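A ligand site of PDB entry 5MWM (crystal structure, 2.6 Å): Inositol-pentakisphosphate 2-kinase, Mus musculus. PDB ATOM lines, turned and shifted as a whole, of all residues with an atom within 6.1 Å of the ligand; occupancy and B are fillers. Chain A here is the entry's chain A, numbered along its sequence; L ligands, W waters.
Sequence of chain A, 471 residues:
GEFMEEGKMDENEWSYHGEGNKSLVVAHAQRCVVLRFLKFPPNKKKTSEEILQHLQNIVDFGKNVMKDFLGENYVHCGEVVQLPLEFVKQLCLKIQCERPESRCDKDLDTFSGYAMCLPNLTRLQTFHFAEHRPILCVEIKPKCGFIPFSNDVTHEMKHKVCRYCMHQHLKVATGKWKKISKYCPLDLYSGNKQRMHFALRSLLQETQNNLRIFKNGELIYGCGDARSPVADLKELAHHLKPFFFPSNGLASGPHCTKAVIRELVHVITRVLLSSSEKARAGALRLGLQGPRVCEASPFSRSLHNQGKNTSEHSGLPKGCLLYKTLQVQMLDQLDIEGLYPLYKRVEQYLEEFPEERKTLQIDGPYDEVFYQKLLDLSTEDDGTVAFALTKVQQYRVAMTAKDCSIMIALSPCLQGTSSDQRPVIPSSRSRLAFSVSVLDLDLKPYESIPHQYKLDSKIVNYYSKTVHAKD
NZ of Lys 444 is in salt-bridge range of O6 of the ligand.
The backbone NH (N) of Asn 21 sits at hydrogen-bond distance from an oxygen (O11) of the ligand (3.2 Å).
An oxygen (O8) of the ligand lies close to the side-chain amide oxygen (OD1) of Asn 21 (2.6 Å).
An oxygen (O20) of the ligand is in salt-bridge range of the side-chain amino group (NZ) of Lys 171.
The side-chain amide nitrogen of Gln 452 is in hydrogen-bond range of an oxygen (O3) of the ligand (2.7 Å).
The side-chain amide nitrogen (ND2) of Asn 209 is in hydrogen-bond range of an oxygen (O14) of the ligand (2.7 Å).
The guanidinium group (NH2) of Arg 103 is in salt-bridge range of an oxygen (O16) of the ligand, at 2.7 Å.
The side-chain amino group (NZ) of Lys 143 is in salt-bridge range of an oxygen (O18) of the ligand (2.8 Å).
NZ of Lys 22 is in salt-bridge range of O7 of the ligand, at 3.3 Å.
The side-chain amino group (NZ) of Lys 141 lies within salt-bridge range of an oxygen (O18) of the ligand (3.2 Å).
An oxygen (O15) of the ligand is in salt-bridge range of the side-chain amino group (NZ) of Lys 176 (3.5 Å).
O24 of the ligand is in salt-bridge range of NH2 of Arg 163, 3.8 Å away.
OD2 of Asp 403 is in salt-bridge range of NZ of Lys 444 (3.2 Å).
The backbone carbonyl oxygen of Lys 171 sits at hydrogen-bond distance from the backbone NH of Lys 176, 2.9 Å away.
The side-chain amide nitrogen of Asn 210 is in hydrogen-bond range of the side-chain amide oxygen of Asn 209 (3.1 Å).
The side-chain amino group (NZ) of Lys 143 is in salt-bridge range of the side-chain carboxylate (OD1) of Asp 403 (3.5 Å).
NZ of Lys 141 lies within salt-bridge range of OD1 of Asp 403 (2.6 Å).
O of Lys 141 sits close to OD1 of Asn 210.
OD2 of Asp 403 sits close to O9 of the ligand, 3.1 Å away.
CA of Gly 20 touches O11 of the ligand (3.6 Å).
CE1 of His 167 touches O22 of the ligand, 3.3 Å away.
Asp 440 touches the ligand.
Leu 455 touches the ligand (CD2 to O23, 3.8 Å).
Hydrophobic or aromatic side chains that line the ligand: His 167 and Leu 455.
Within 4 Å of the ligand: Gly 20, Asn 21, Lys 22, Arg 103, Lys 141, Lys 143, Arg 163, His 167, Lys 171, Lys 176, Asn 209, Asp 403, Asp 440, Lys 444, Gln 452 and Leu 455.
The nearest printed residue that does not touch the ligand is Met 399 (4.1 Å).
Water W1 lies within hydrogen-bond range of the guanidinium group (NE) of Arg 163, an oxygen (O24) of the ligand and a ring nitrogen (ND1) of His 167.
Water W2 bridges NZ of Lys 171 (2.8 Å) and O20 of the ligand (2.9 Å).
Water W3 lies within hydrogen-bond range of the side-chain carboxylate (OD1) of Asp 440 (2.9 Å), an oxygen (O12) of the ligand (3.1 Å) and the side-chain hydroxyl (OG) of Ser 23 (3.4 Å).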
ATOM      1  N   GLU A  19      -0.628 -29.628 -27.928  1.00  0.00           N
ATOM      2  CA  GLU A  19      -0.155 -28.310 -27.517  1.00  0.00           C
ATOM      3  C   GLU A  19      -1.292 -27.291 -27.327  1.00  0.00           C
ATOM      4  O   GLU A  19      -2.426 -27.533 -27.740  1.00  0.00           O
ATOM      5  CB  GLU A  19       0.907 -27.773 -28.490  1.00  0.00           C
ATOM      6  CG  GLU A  19       0.378 -27.182 -29.781  1.00  0.00           C
ATOM      7  CD  GLU A  19       1.433 -27.114 -30.880  1.00  0.00           C
ATOM      8  OE1 GLU A  19       1.862 -25.993 -31.244  1.00  0.00           O
ATOM      9  OE2 GLU A  19       1.817 -28.192 -31.389  1.00  0.00           O
ATOM     10  N   GLY A  20      -0.958 -26.198 -26.656  1.00  0.00           N
ATOM     11  CA  GLY A  20      -1.712 -24.936 -26.666  1.00  0.00           C
ATOM     12  C   GLY A  20      -0.769 -23.886 -27.225  1.00  0.00           C
ATOM     13  O   GLY A  20       0.251 -24.244 -27.829  1.00  0.00           O
ATOM     14  N   ASN A  21      -1.082 -22.603 -27.057  1.00  0.00           N
ATOM     15  CA  ASN A  21      -0.190 -21.530 -27.565  1.00  0.00           C
ATOM     16  C   ASN A  21       0.904 -21.090 -26.582  1.00  0.00           C
ATOM     17  O   ASN A  21       1.799 -20.342 -26.967  1.00  0.00           O
ATOM     18  CB  ASN A  21      -0.988 -20.306 -28.040  1.00  0.00           C
ATOM     19  CG  ASN A  21      -1.680 -19.560 -26.913  1.00  0.00           C
ATOM     20  OD1 ASN A  21      -1.880 -20.113 -25.826  1.00  0.00           O
ATOM     21  ND2 ASN A  21      -2.063 -18.320 -27.160  1.00  0.00           N
ATOM     22  N   LYS A  22       0.821 -21.543 -25.327  1.00  0.00           N
ATOM     23  CA  LYS A  22       1.861 -21.266 -24.327  1.00  0.00           C
ATOM     24  C   LYS A  22       2.919 -22.367 -24.229  1.00  0.00           C
ATOM     25  O   LYS A  22       4.068 -22.072 -23.900  1.00  0.00           O
ATOM     26  CB  LYS A  22       1.229 -21.032 -22.941  1.00  0.00           C
ATOM     27  CG  LYS A  22       1.296 -19.602 -22.407  1.00  0.00           C
ATOM     28  CD  LYS A  22       1.110 -18.512 -23.455  1.00  0.00           C
ATOM     29  CE  LYS A  22       0.906 -17.151 -22.808  1.00  0.00           C
ATOM     30  NZ  LYS A  22       0.716 -16.070 -23.816  1.00  0.00           N
ATOM     31  N   SER A  23       2.531 -23.603 -24.516  1.00  0.00           N
ATOM     32  CA  SER A  23       3.418 -24.749 -24.319  1.00  0.00           C
ATOM     33  C   SER A  23       3.247 -25.829 -25.383  1.00  0.00           C
ATOM     34  O   SER A  23       2.362 -25.727 -26.223  1.00  0.00           O
ATOM     35  CB  SER A  23       3.135 -25.357 -22.954  1.00  0.00           C
ATOM     36  OG  SER A  23       1.789 -25.808 -22.883  1.00  0.00           O
ATOM     37  N   ARG A 103      -1.187 -23.708 -35.216  1.00  0.00           N
ATOM     38  CA  ARG A 103      -0.185 -23.395 -34.190  1.00  0.00           C
ATOM     39  C   ARG A 103       1.279 -23.465 -34.657  1.00  0.00           C
ATOM     40  O   ARG A 103       2.196 -23.555 -33.831  1.00  0.00           O
ATOM     41  CB  ARG A 103      -0.396 -24.315 -32.991  1.00  0.00           C
ATOM     42  CG  ARG A 103      -1.772 -24.221 -32.372  1.00  0.00           C
ATOM     43  CD  ARG A 103      -1.791 -24.993 -31.077  1.00  0.00           C
ATOM     44  NE  ARG A 103      -3.087 -24.942 -30.406  1.00  0.00           N
ATOM     45  CZ  ARG A 103      -3.552 -23.912 -29.704  1.00  0.00           C
ATOM     46  NH1 ARG A 103      -2.864 -22.776 -29.587  1.00  0.00           N
ATOM     47  NH2 ARG A 103      -4.735 -24.017 -29.133  1.00  0.00           N
ATOM     48  N   LYS A 141     -11.579 -28.975 -21.048  1.00  0.00           N
ATOM     49  CA  LYS A 141     -11.251 -27.589 -20.748  1.00  0.00           C
ATOM     50  C   LYS A 141     -12.600 -26.930 -20.469  1.00  0.00           C
ATOM     51  O   LYS A 141     -13.216 -26.374 -21.383  1.00  0.00           O
ATOM     52  CB  LYS A 141     -10.549 -26.952 -21.935  1.00  0.00           C
ATOM     53  CG  LYS A 141      -9.666 -25.768 -21.579  1.00  0.00           C
ATOM     54  CD  LYS A 141      -9.496 -24.793 -22.744  1.00  0.00           C
ATOM     55  CE  LYS A 141      -8.092 -24.195 -22.773  1.00  0.00           C
ATOM     56  NZ  LYS A 141      -8.110 -22.812 -23.302  1.00  0.00           N
ATOM     57  N   LYS A 143     -13.775 -24.330 -18.881  1.00  0.00           N
ATOM     58  CA  LYS A 143     -13.863 -22.869 -18.955  1.00  0.00           C
ATOM     59  C   LYS A 143     -14.651 -22.335 -17.748  1.00  0.00           C
ATOM     60  O   LYS A 143     -14.722 -23.028 -16.741  1.00  0.00           O
ATOM     61  CB  LYS A 143     -14.357 -22.390 -20.330  1.00  0.00           C
ATOM     62  CG  LYS A 143     -13.514 -22.938 -21.484  1.00  0.00           C
ATOM     63  CD  LYS A 143     -12.655 -21.885 -22.181  1.00  0.00           C
ATOM     64  CE  LYS A 143     -11.630 -21.229 -21.256  1.00  0.00           C
ATOM     65  NZ  LYS A 143     -10.904 -20.147 -21.972  1.00  0.00           N
ATOM     66  N   ARG A 163     -19.740 -16.138 -20.270  1.00  0.00           N
ATOM     67  CA  ARG A 163     -18.622 -15.745 -21.153  1.00  0.00           C
ATOM     68  C   ARG A 163     -18.468 -16.683 -22.345  1.00  0.00           C
ATOM     69  O   ARG A 163     -18.427 -16.237 -23.507  1.00  0.00           O
ATOM     70  CB  ARG A 163     -17.315 -15.690 -20.338  1.00  0.00           C
ATOM     71  CG  ARG A 163     -15.998 -15.711 -21.115  1.00  0.00           C
ATOM     72  CD  ARG A 163     -15.842 -14.570 -22.113  1.00  0.00           C
ATOM     73  NE  ARG A 163     -14.413 -14.386 -22.394  1.00  0.00           N
ATOM     74  CZ  ARG A 163     -13.603 -13.449 -21.873  1.00  0.00           C
ATOM     75  NH1 ARG A 163     -14.054 -12.508 -21.046  1.00  0.00           N
ATOM     76  NH2 ARG A 163     -12.315 -13.451 -22.221  1.00  0.00           N
ATOM     77  N   HIS A 167     -18.806 -15.773 -26.392  1.00  0.00           N
ATOM     78  CA  HIS A 167     -17.528 -15.910 -27.149  1.00  0.00           C
ATOM     79  C   HIS A 167     -17.680 -16.743 -28.426  1.00  0.00           C
ATOM     80  O   HIS A 167     -17.291 -16.308 -29.521  1.00  0.00           O
ATOM     81  CB  HIS A 167     -16.448 -16.565 -26.269  1.00  0.00           C
ATOM     82  CG  HIS A 167     -15.055 -16.209 -26.671  1.00  0.00           C
ATOM     83  ND1 HIS A 167     -14.005 -16.228 -25.778  1.00  0.00           N
ATOM     84  CD2 HIS A 167     -14.533 -15.778 -27.847  1.00  0.00           C
ATOM     85  CE1 HIS A 167     -12.901 -15.850 -26.391  1.00  0.00           C
ATOM     86  NE2 HIS A 167     -13.193 -15.568 -27.645  1.00  0.00           N
ATOM     87  N   LYS A 171     -15.792 -16.564 -32.342  1.00  0.00           N
ATOM     88  CA  LYS A 171     -14.874 -17.619 -32.832  1.00  0.00           C
ATOM     89  C   LYS A 171     -15.294 -18.180 -34.177  1.00  0.00           C
ATOM     90  O   LYS A 171     -14.461 -18.361 -35.067  1.00  0.00           O
ATOM     91  CB  LYS A 171     -14.760 -18.754 -31.811  1.00  0.00           C
ATOM     92  CG  LYS A 171     -14.047 -18.355 -30.532  1.00  0.00           C
ATOM     93  CD  LYS A 171     -14.140 -19.427 -29.464  1.00  0.00           C
ATOM     94  CE  LYS A 171     -13.120 -19.181 -28.357  1.00  0.00           C
ATOM     95  NZ  LYS A 171     -13.401 -19.928 -27.102  1.00  0.00           N
ATOM     96  N   LYS A 176     -12.300 -19.642 -36.427  1.00  0.00           N
ATOM     97  CA  LYS A 176     -11.488 -20.501 -35.554  1.00  0.00           C
ATOM     98  C   LYS A 176     -12.130 -21.897 -35.548  1.00  0.00           C
ATOM     99  O   LYS A 176     -11.430 -22.904 -35.677  1.00  0.00           O
ATOM    100  CB  LYS A 176     -11.426 -19.918 -34.136  1.00  0.00           C
ATOM    101  CG  LYS A 176     -10.668 -20.755 -33.113  1.00  0.00           C
ATOM    102  CD  LYS A 176     -10.581 -20.063 -31.753  1.00  0.00           C
ATOM    103  CE  LYS A 176      -9.389 -19.111 -31.662  1.00  0.00           C
ATOM    104  NZ  LYS A 176      -8.089 -19.811 -31.465  1.00  0.00           N
ATOM    105  N   TRP A 177     -13.460 -21.929 -35.387  1.00  0.00           N
ATOM    106  CA  TRP A 177     -14.246 -23.173 -35.430  1.00  0.00           C
ATOM    107  C   TRP A 177     -15.371 -23.077 -36.448  1.00  0.00           C
ATOM    108  O   TRP A 177     -15.802 -21.981 -36.812  1.00  0.00           O
ATOM    109  CB  TRP A 177     -14.790 -23.509 -34.033  1.00  0.00           C
ATOM    110  CG  TRP A 177     -13.683 -23.675 -33.039  1.00  0.00           C
ATOM    111  CD1 TRP A 177     -13.448 -22.910 -31.944  1.00  0.00           C
ATOM    112  CD2 TRP A 177     -12.621 -24.632 -33.105  1.00  0.00           C
ATOM    113  NE1 TRP A 177     -12.324 -23.337 -31.296  1.00  0.00           N
ATOM    114  CE2 TRP A 177     -11.795 -24.391 -31.994  1.00  0.00           C
ATOM    115  CE3 TRP A 177     -12.304 -25.676 -33.981  1.00  0.00           C
ATOM    116  CZ2 TRP A 177     -10.656 -25.171 -31.736  1.00  0.00           C
ATOM    117  CZ3 TRP A 177     -11.176 -26.445 -33.729  1.00  0.00           C
ATOM    118  CH2 TRP A 177     -10.362 -26.187 -32.610  1.00  0.00           C
ATOM    119  N   ASN A 209     -11.617 -27.091 -28.661  1.00  0.00           N
ATOM    120  CA  ASN A 209     -10.464 -27.278 -27.773  1.00  0.00           C
ATOM    121  C   ASN A 209     -10.947 -27.543 -26.359  1.00  0.00           C
ATOM    122  O   ASN A 209     -10.257 -27.197 -25.385  1.00  0.00           O
ATOM    123  CB  ASN A 209      -9.567 -26.023 -27.805  1.00  0.00           C
ATOM    124  CG  ASN A 209     -10.263 -24.777 -27.251  1.00  0.00           C
ATOM    125  OD1 ASN A 209     -11.495 -24.689 -27.235  1.00  0.00           O
ATOM    126  ND2 ASN A 209      -9.477 -23.814 -26.796  1.00  0.00           N
ATOM    127  N   ASN A 210     -12.131 -28.135 -26.232  1.00  0.00           N
ATOM    128  CA  ASN A 210     -12.755 -28.372 -24.937  1.00  0.00           C
ATOM    129  C   ASN A 210     -12.934 -29.851 -24.592  1.00  0.00           C
ATOM    130  O   ASN A 210     -13.351 -30.168 -23.475  1.00  0.00           O
ATOM    131  CB  ASN A 210     -14.082 -27.599 -24.846  1.00  0.00           C
ATOM    132  CG  ASN A 210     -13.888 -26.094 -25.023  1.00  0.00           C
ATOM    133  OD1 ASN A 210     -13.358 -25.422 -24.139  1.00  0.00           O
ATOM    134  ND2 ASN A 210     -14.284 -25.578 -26.172  1.00  0.00           N
ATOM    135  N   MET A 399      -8.269 -16.348 -13.254  1.00  0.00           N
ATOM    136  CA  MET A 399      -7.945 -16.418 -14.685  1.00  0.00           C
ATOM    137  C   MET A 399      -7.218 -17.730 -15.036  1.00  0.00           C
ATOM    138  O   MET A 399      -7.432 -18.271 -16.122  1.00  0.00           O
ATOM    139  CB  MET A 399      -7.006 -15.244 -15.030  1.00  0.00           C
ATOM    140  CG  MET A 399      -7.168 -14.590 -16.385  1.00  0.00           C
ATOM    141  SD  MET A 399      -6.245 -13.030 -16.291  1.00  0.00           S
ATOM    142  CE  MET A 399      -5.476 -12.967 -17.902  1.00  0.00           C
ATOM    143  N   ASP A 403      -8.873 -21.254 -17.259  1.00  0.00           N
ATOM    144  CA  ASP A 403      -8.304 -21.788 -18.504  1.00  0.00           C
ATOM    145  C   ASP A 403      -7.689 -23.179 -18.323  1.00  0.00           C
ATOM    146  O   ASP A 403      -6.982 -23.650 -19.217  1.00  0.00           O
ATOM    147  CB  ASP A 403      -7.253 -20.820 -19.039  1.00  0.00           C
ATOM    148  CG  ASP A 403      -6.782 -21.191 -20.459  1.00  0.00           C
ATOM    149  OD1 ASP A 403      -7.602 -21.097 -21.398  1.00  0.00           O
ATOM    150  OD2 ASP A 403      -5.597 -21.573 -20.607  1.00  0.00           O
ATOM    151  N   SER A 405      -7.324 -27.361 -17.741  1.00  0.00           N
ATOM    152  CA  SER A 405      -7.929 -28.620 -18.211  1.00  0.00           C
ATOM    153  C   SER A 405      -8.001 -29.661 -17.104  1.00  0.00           C
ATOM    154  O   SER A 405      -7.209 -29.619 -16.156  1.00  0.00           O
ATOM    155  CB  SER A 405      -7.142 -29.176 -19.395  1.00  0.00           C
ATOM    156  OG  SER A 405      -7.145 -28.278 -20.488  1.00  0.00           O
ATOM    157  N   ASP A 440      -2.654 -27.406 -17.052  1.00  0.00           N
ATOM    158  CA  ASP A 440      -2.531 -26.009 -17.507  1.00  0.00           C
ATOM    159  C   ASP A 440      -2.618 -25.018 -16.329  1.00  0.00           C
ATOM    160  O   ASP A 440      -3.365 -24.032 -16.369  1.00  0.00           O
ATOM    161  CB  ASP A 440      -3.576 -25.709 -18.621  1.00  0.00           C
ATOM    162  CG  ASP A 440      -3.009 -25.875 -20.035  1.00  0.00           C
ATOM    163  OD1 ASP A 440      -1.988 -25.236 -20.352  1.00  0.00           O
ATOM    164  OD2 ASP A 440      -3.611 -26.612 -20.856  1.00  0.00           O
ATOM    165  N   ASP A 442      -0.374 -22.774 -14.895  1.00  0.00           N
ATOM    166  CA  ASP A 442       0.665 -21.742 -14.800  1.00  0.00           C
ATOM    167  C   ASP A 442      -0.018 -20.388 -14.738  1.00  0.00           C
ATOM    168  O   ASP A 442      -1.022 -20.159 -15.416  1.00  0.00           O
ATOM    169  CB  ASP A 442       1.674 -21.824 -15.952  1.00  0.00           C
ATOM    170  CG  ASP A 442       1.049 -21.612 -17.309  1.00  0.00           C
ATOM    171  OD1 ASP A 442      -0.100 -22.039 -17.523  1.00  0.00           O
ATOM    172  OD2 ASP A 442       1.736 -21.031 -18.190  1.00  0.00           O
ATOM    173  N   LYS A 444      -1.320 -16.739 -15.124  1.00  0.00           N
ATOM    174  CA  LYS A 444      -1.450 -15.755 -16.186  1.00  0.00           C
ATOM    175  C   LYS A 444      -0.667 -14.520 -15.813  1.00  0.00           C
ATOM    176  O   LYS A 444      -0.660 -14.122 -14.644  1.00  0.00           O
ATOM    177  CB  LYS A 444      -2.909 -15.382 -16.418  1.00  0.00           C
ATOM    178  CG  LYS A 444      -3.828 -16.547 -16.756  1.00  0.00           C
ATOM    179  CD  LYS A 444      -3.245 -17.462 -17.828  1.00  0.00           C
ATOM    180  CE  LYS A 444      -4.216 -18.554 -18.224  1.00  0.00           C
ATOM    181  NZ  LYS A 444      -3.920 -19.048 -19.594  1.00  0.00           N
ATOM    182  N   PRO A 445       0.010 -13.902 -16.799  1.00  0.00           N
ATOM    183  CA  PRO A 445       0.805 -12.729 -16.455  1.00  0.00           C
ATOM    184  C   PRO A 445      -0.021 -11.490 -16.059  1.00  0.00           C
ATOM    185  O   PRO A 445      -1.113 -11.276 -16.595  1.00  0.00           O
ATOM    186  CB  PRO A 445       1.635 -12.467 -17.723  1.00  0.00           C
ATOM    187  CG  PRO A 445       0.995 -13.253 -18.814  1.00  0.00           C
ATOM    188  CD  PRO A 445       0.243 -14.372 -18.173  1.00  0.00           C
ATOM    189  N   SER A 448      -1.023  -9.049 -19.067  1.00  0.00           N
ATOM    190  CA  SER A 448      -2.096  -9.382 -20.008  1.00  0.00           C
ATOM    191  C   SER A 448      -3.499  -8.954 -19.565  1.00  0.00           C
ATOM    192  O   SER A 448      -4.468  -9.292 -20.212  1.00  0.00           O
ATOM    193  CB  SER A 448      -2.122 -10.906 -20.228  1.00  0.00           C
ATOM    194  OG  SER A 448      -2.594 -11.566 -19.068  1.00  0.00           O
ATOM    195  N   HIS A 451      -5.285  -6.682 -22.114  1.00  0.00           N
ATOM    196  CA  HIS A 451      -5.811  -7.491 -23.208  1.00  0.00           C
ATOM    197  C   HIS A 451      -7.176  -8.097 -22.857  1.00  0.00           C
ATOM    198  O   HIS A 451      -8.080  -8.104 -23.685  1.00  0.00           O
ATOM    199  CB  HIS A 451      -4.810  -8.591 -23.592  1.00  0.00           C
ATOM    200  CG  HIS A 451      -5.369  -9.620 -24.538  1.00  0.00           C
ATOM    201  ND1 HIS A 451      -5.719  -9.315 -25.840  1.00  0.00           N
ATOM    202  CD2 HIS A 451      -5.648 -10.927 -24.362  1.00  0.00           C
ATOM    203  CE1 HIS A 451      -6.186 -10.403 -26.430  1.00  0.00           C
ATOM    204  NE2 HIS A 451      -6.152 -11.398 -25.548  1.00  0.00           N
ATOM    205  N   GLN A 452      -7.310  -8.602 -21.631  1.00  0.00           N
ATOM    206  CA  GLN A 452      -8.575  -9.170 -21.155  1.00  0.00           C
ATOM    207  C   GLN A 452      -9.704  -8.138 -21.036  1.00  0.00           C
ATOM    208  O   GLN A 452     -10.869  -8.493 -21.194  1.00  0.00           O
ATOM    209  CB  GLN A 452      -8.397  -9.864 -19.806  1.00  0.00           C
ATOM    210  CG  GLN A 452      -7.490 -11.073 -19.849  1.00  0.00           C
ATOM    211  CD  GLN A 452      -8.051 -12.193 -20.695  1.00  0.00           C
ATOM    212  OE1 GLN A 452      -9.231 -12.534 -20.603  1.00  0.00           O
ATOM    213  NE2 GLN A 452      -7.204 -12.768 -21.550  1.00  0.00           N
ATOM    214  N   LEU A 455     -10.687  -7.404 -24.815  1.00  0.00           N
ATOM    215  CA  LEU A 455     -11.341  -8.590 -25.365  1.00  0.00           C
ATOM    216  C   LEU A 455     -12.757  -8.768 -24.802  1.00  0.00           C
ATOM    217  O   LEU A 455     -13.650  -9.238 -25.518  1.00  0.00           O
ATOM    218  CB  LEU A 455     -10.487  -9.822 -25.068  1.00  0.00           C
ATOM    219  CG  LEU A 455     -10.878 -11.150 -25.710  1.00  0.00           C
ATOM    220  CD1 LEU A 455     -10.997 -11.008 -27.219  1.00  0.00           C
ATOM    221  CD2 LEU A 455      -9.842 -12.200 -25.345  1.00  0.00           C
HETATM  222  C1  LIG L   1      -6.229 -18.271 -23.153  1.00  0.00           C
HETATM  223  C2  LIG L   1      -4.956 -18.838 -23.783  1.00  0.00           C
HETATM  224  C3  LIG L   1      -5.198 -20.122 -24.583  1.00  0.00           C
HETATM  225  C4  LIG L   1      -6.458 -20.092 -25.442  1.00  0.00           C
HETATM  226  C5  LIG L   1      -7.684 -19.628 -24.691  1.00  0.00           C
HETATM  227  C6  LIG L   1      -7.449 -18.269 -24.056  1.00  0.00           C
HETATM  228  O1  LIG L   1      -5.936 -16.882 -22.899  1.00  0.00           O
HETATM  229  P1  LIG L   1      -6.096 -16.019 -21.521  1.00  0.00           P
HETATM  230  O2  LIG L   1      -5.042 -14.934 -21.511  1.00  0.00           O
HETATM  231  O3  LIG L   1      -7.501 -15.434 -21.514  1.00  0.00           O
HETATM  232  O4  LIG L   1      -6.006 -16.981 -20.330  1.00  0.00           O
HETATM  233  O5  LIG L   1      -4.023 -19.081 -22.718  1.00  0.00           O
HETATM  234  P2  LIG L   1      -2.464 -18.634 -22.696  1.00  0.00           P
HETATM  235  O6  LIG L   1      -2.042 -18.444 -21.251  1.00  0.00           O
HETATM  236  O7  LIG L   1      -2.229 -17.415 -23.517  1.00  0.00           O
HETATM  237  O8  LIG L   1      -1.765 -19.878 -23.205  1.00  0.00           O
HETATM  238  O9  LIG L   1      -5.177 -21.272 -23.687  1.00  0.00           O
HETATM  239  P3  LIG L   1      -4.298 -22.692 -24.010  1.00  0.00           P
HETATM  240  O10 LIG L   1      -4.986 -23.550 -25.062  1.00  0.00           O
HETATM  241  O11 LIG L   1      -2.862 -22.309 -24.452  1.00  0.00           O
HETATM  242  O12 LIG L   1      -4.159 -23.463 -22.680  1.00  0.00           O
HETATM  243  O13 LIG L   1      -6.729 -21.423 -25.910  1.00  0.00           O
HETATM  244  P4  LIG L   1      -6.642 -21.861 -27.436  1.00  0.00           P
HETATM  245  O14 LIG L   1      -6.905 -23.365 -27.431  1.00  0.00           O
HETATM  246  O15 LIG L   1      -7.601 -21.058 -28.224  1.00  0.00           O
HETATM  247  O16 LIG L   1      -5.182 -21.654 -27.826  1.00  0.00           O
HETATM  248  O17 LIG L   1      -8.748 -19.497 -25.664  1.00  0.00           O
HETATM  249  P5  LIG L   1     -10.192 -20.151 -25.820  1.00  0.00           P
HETATM  250  O18 LIG L   1     -10.451 -21.036 -24.597  1.00  0.00           O
HETATM  251  O19 LIG L   1     -10.167 -21.039 -27.077  1.00  0.00           O
HETATM  252  O20 LIG L   1     -11.167 -19.036 -25.939  1.00  0.00           O
HETATM  253  O21 LIG L   1      -8.603 -17.971 -23.234  1.00  0.00           O
HETATM  254  P6  LIG L   1      -9.674 -16.792 -23.529  1.00  0.00           P
HETATM  255  O22 LIG L   1     -10.329 -17.149 -24.828  1.00  0.00           O
HETATM  256  O23 LIG L   1      -9.044 -15.429 -23.563  1.00  0.00           O
HETATM  257  O24 LIG L   1     -10.742 -16.881 -22.464  1.00  0.00           O
HETATM  258  O   HOH W   1     -13.326 -16.647 -23.038  1.00  0.00           O
HETATM  259  O   HOH W   2     -13.595 -19.460 -24.360  1.00  0.00           O
HETATM  260  O   HOH W   3      -1.482 -24.889 -23.136  1.00  0.00           O
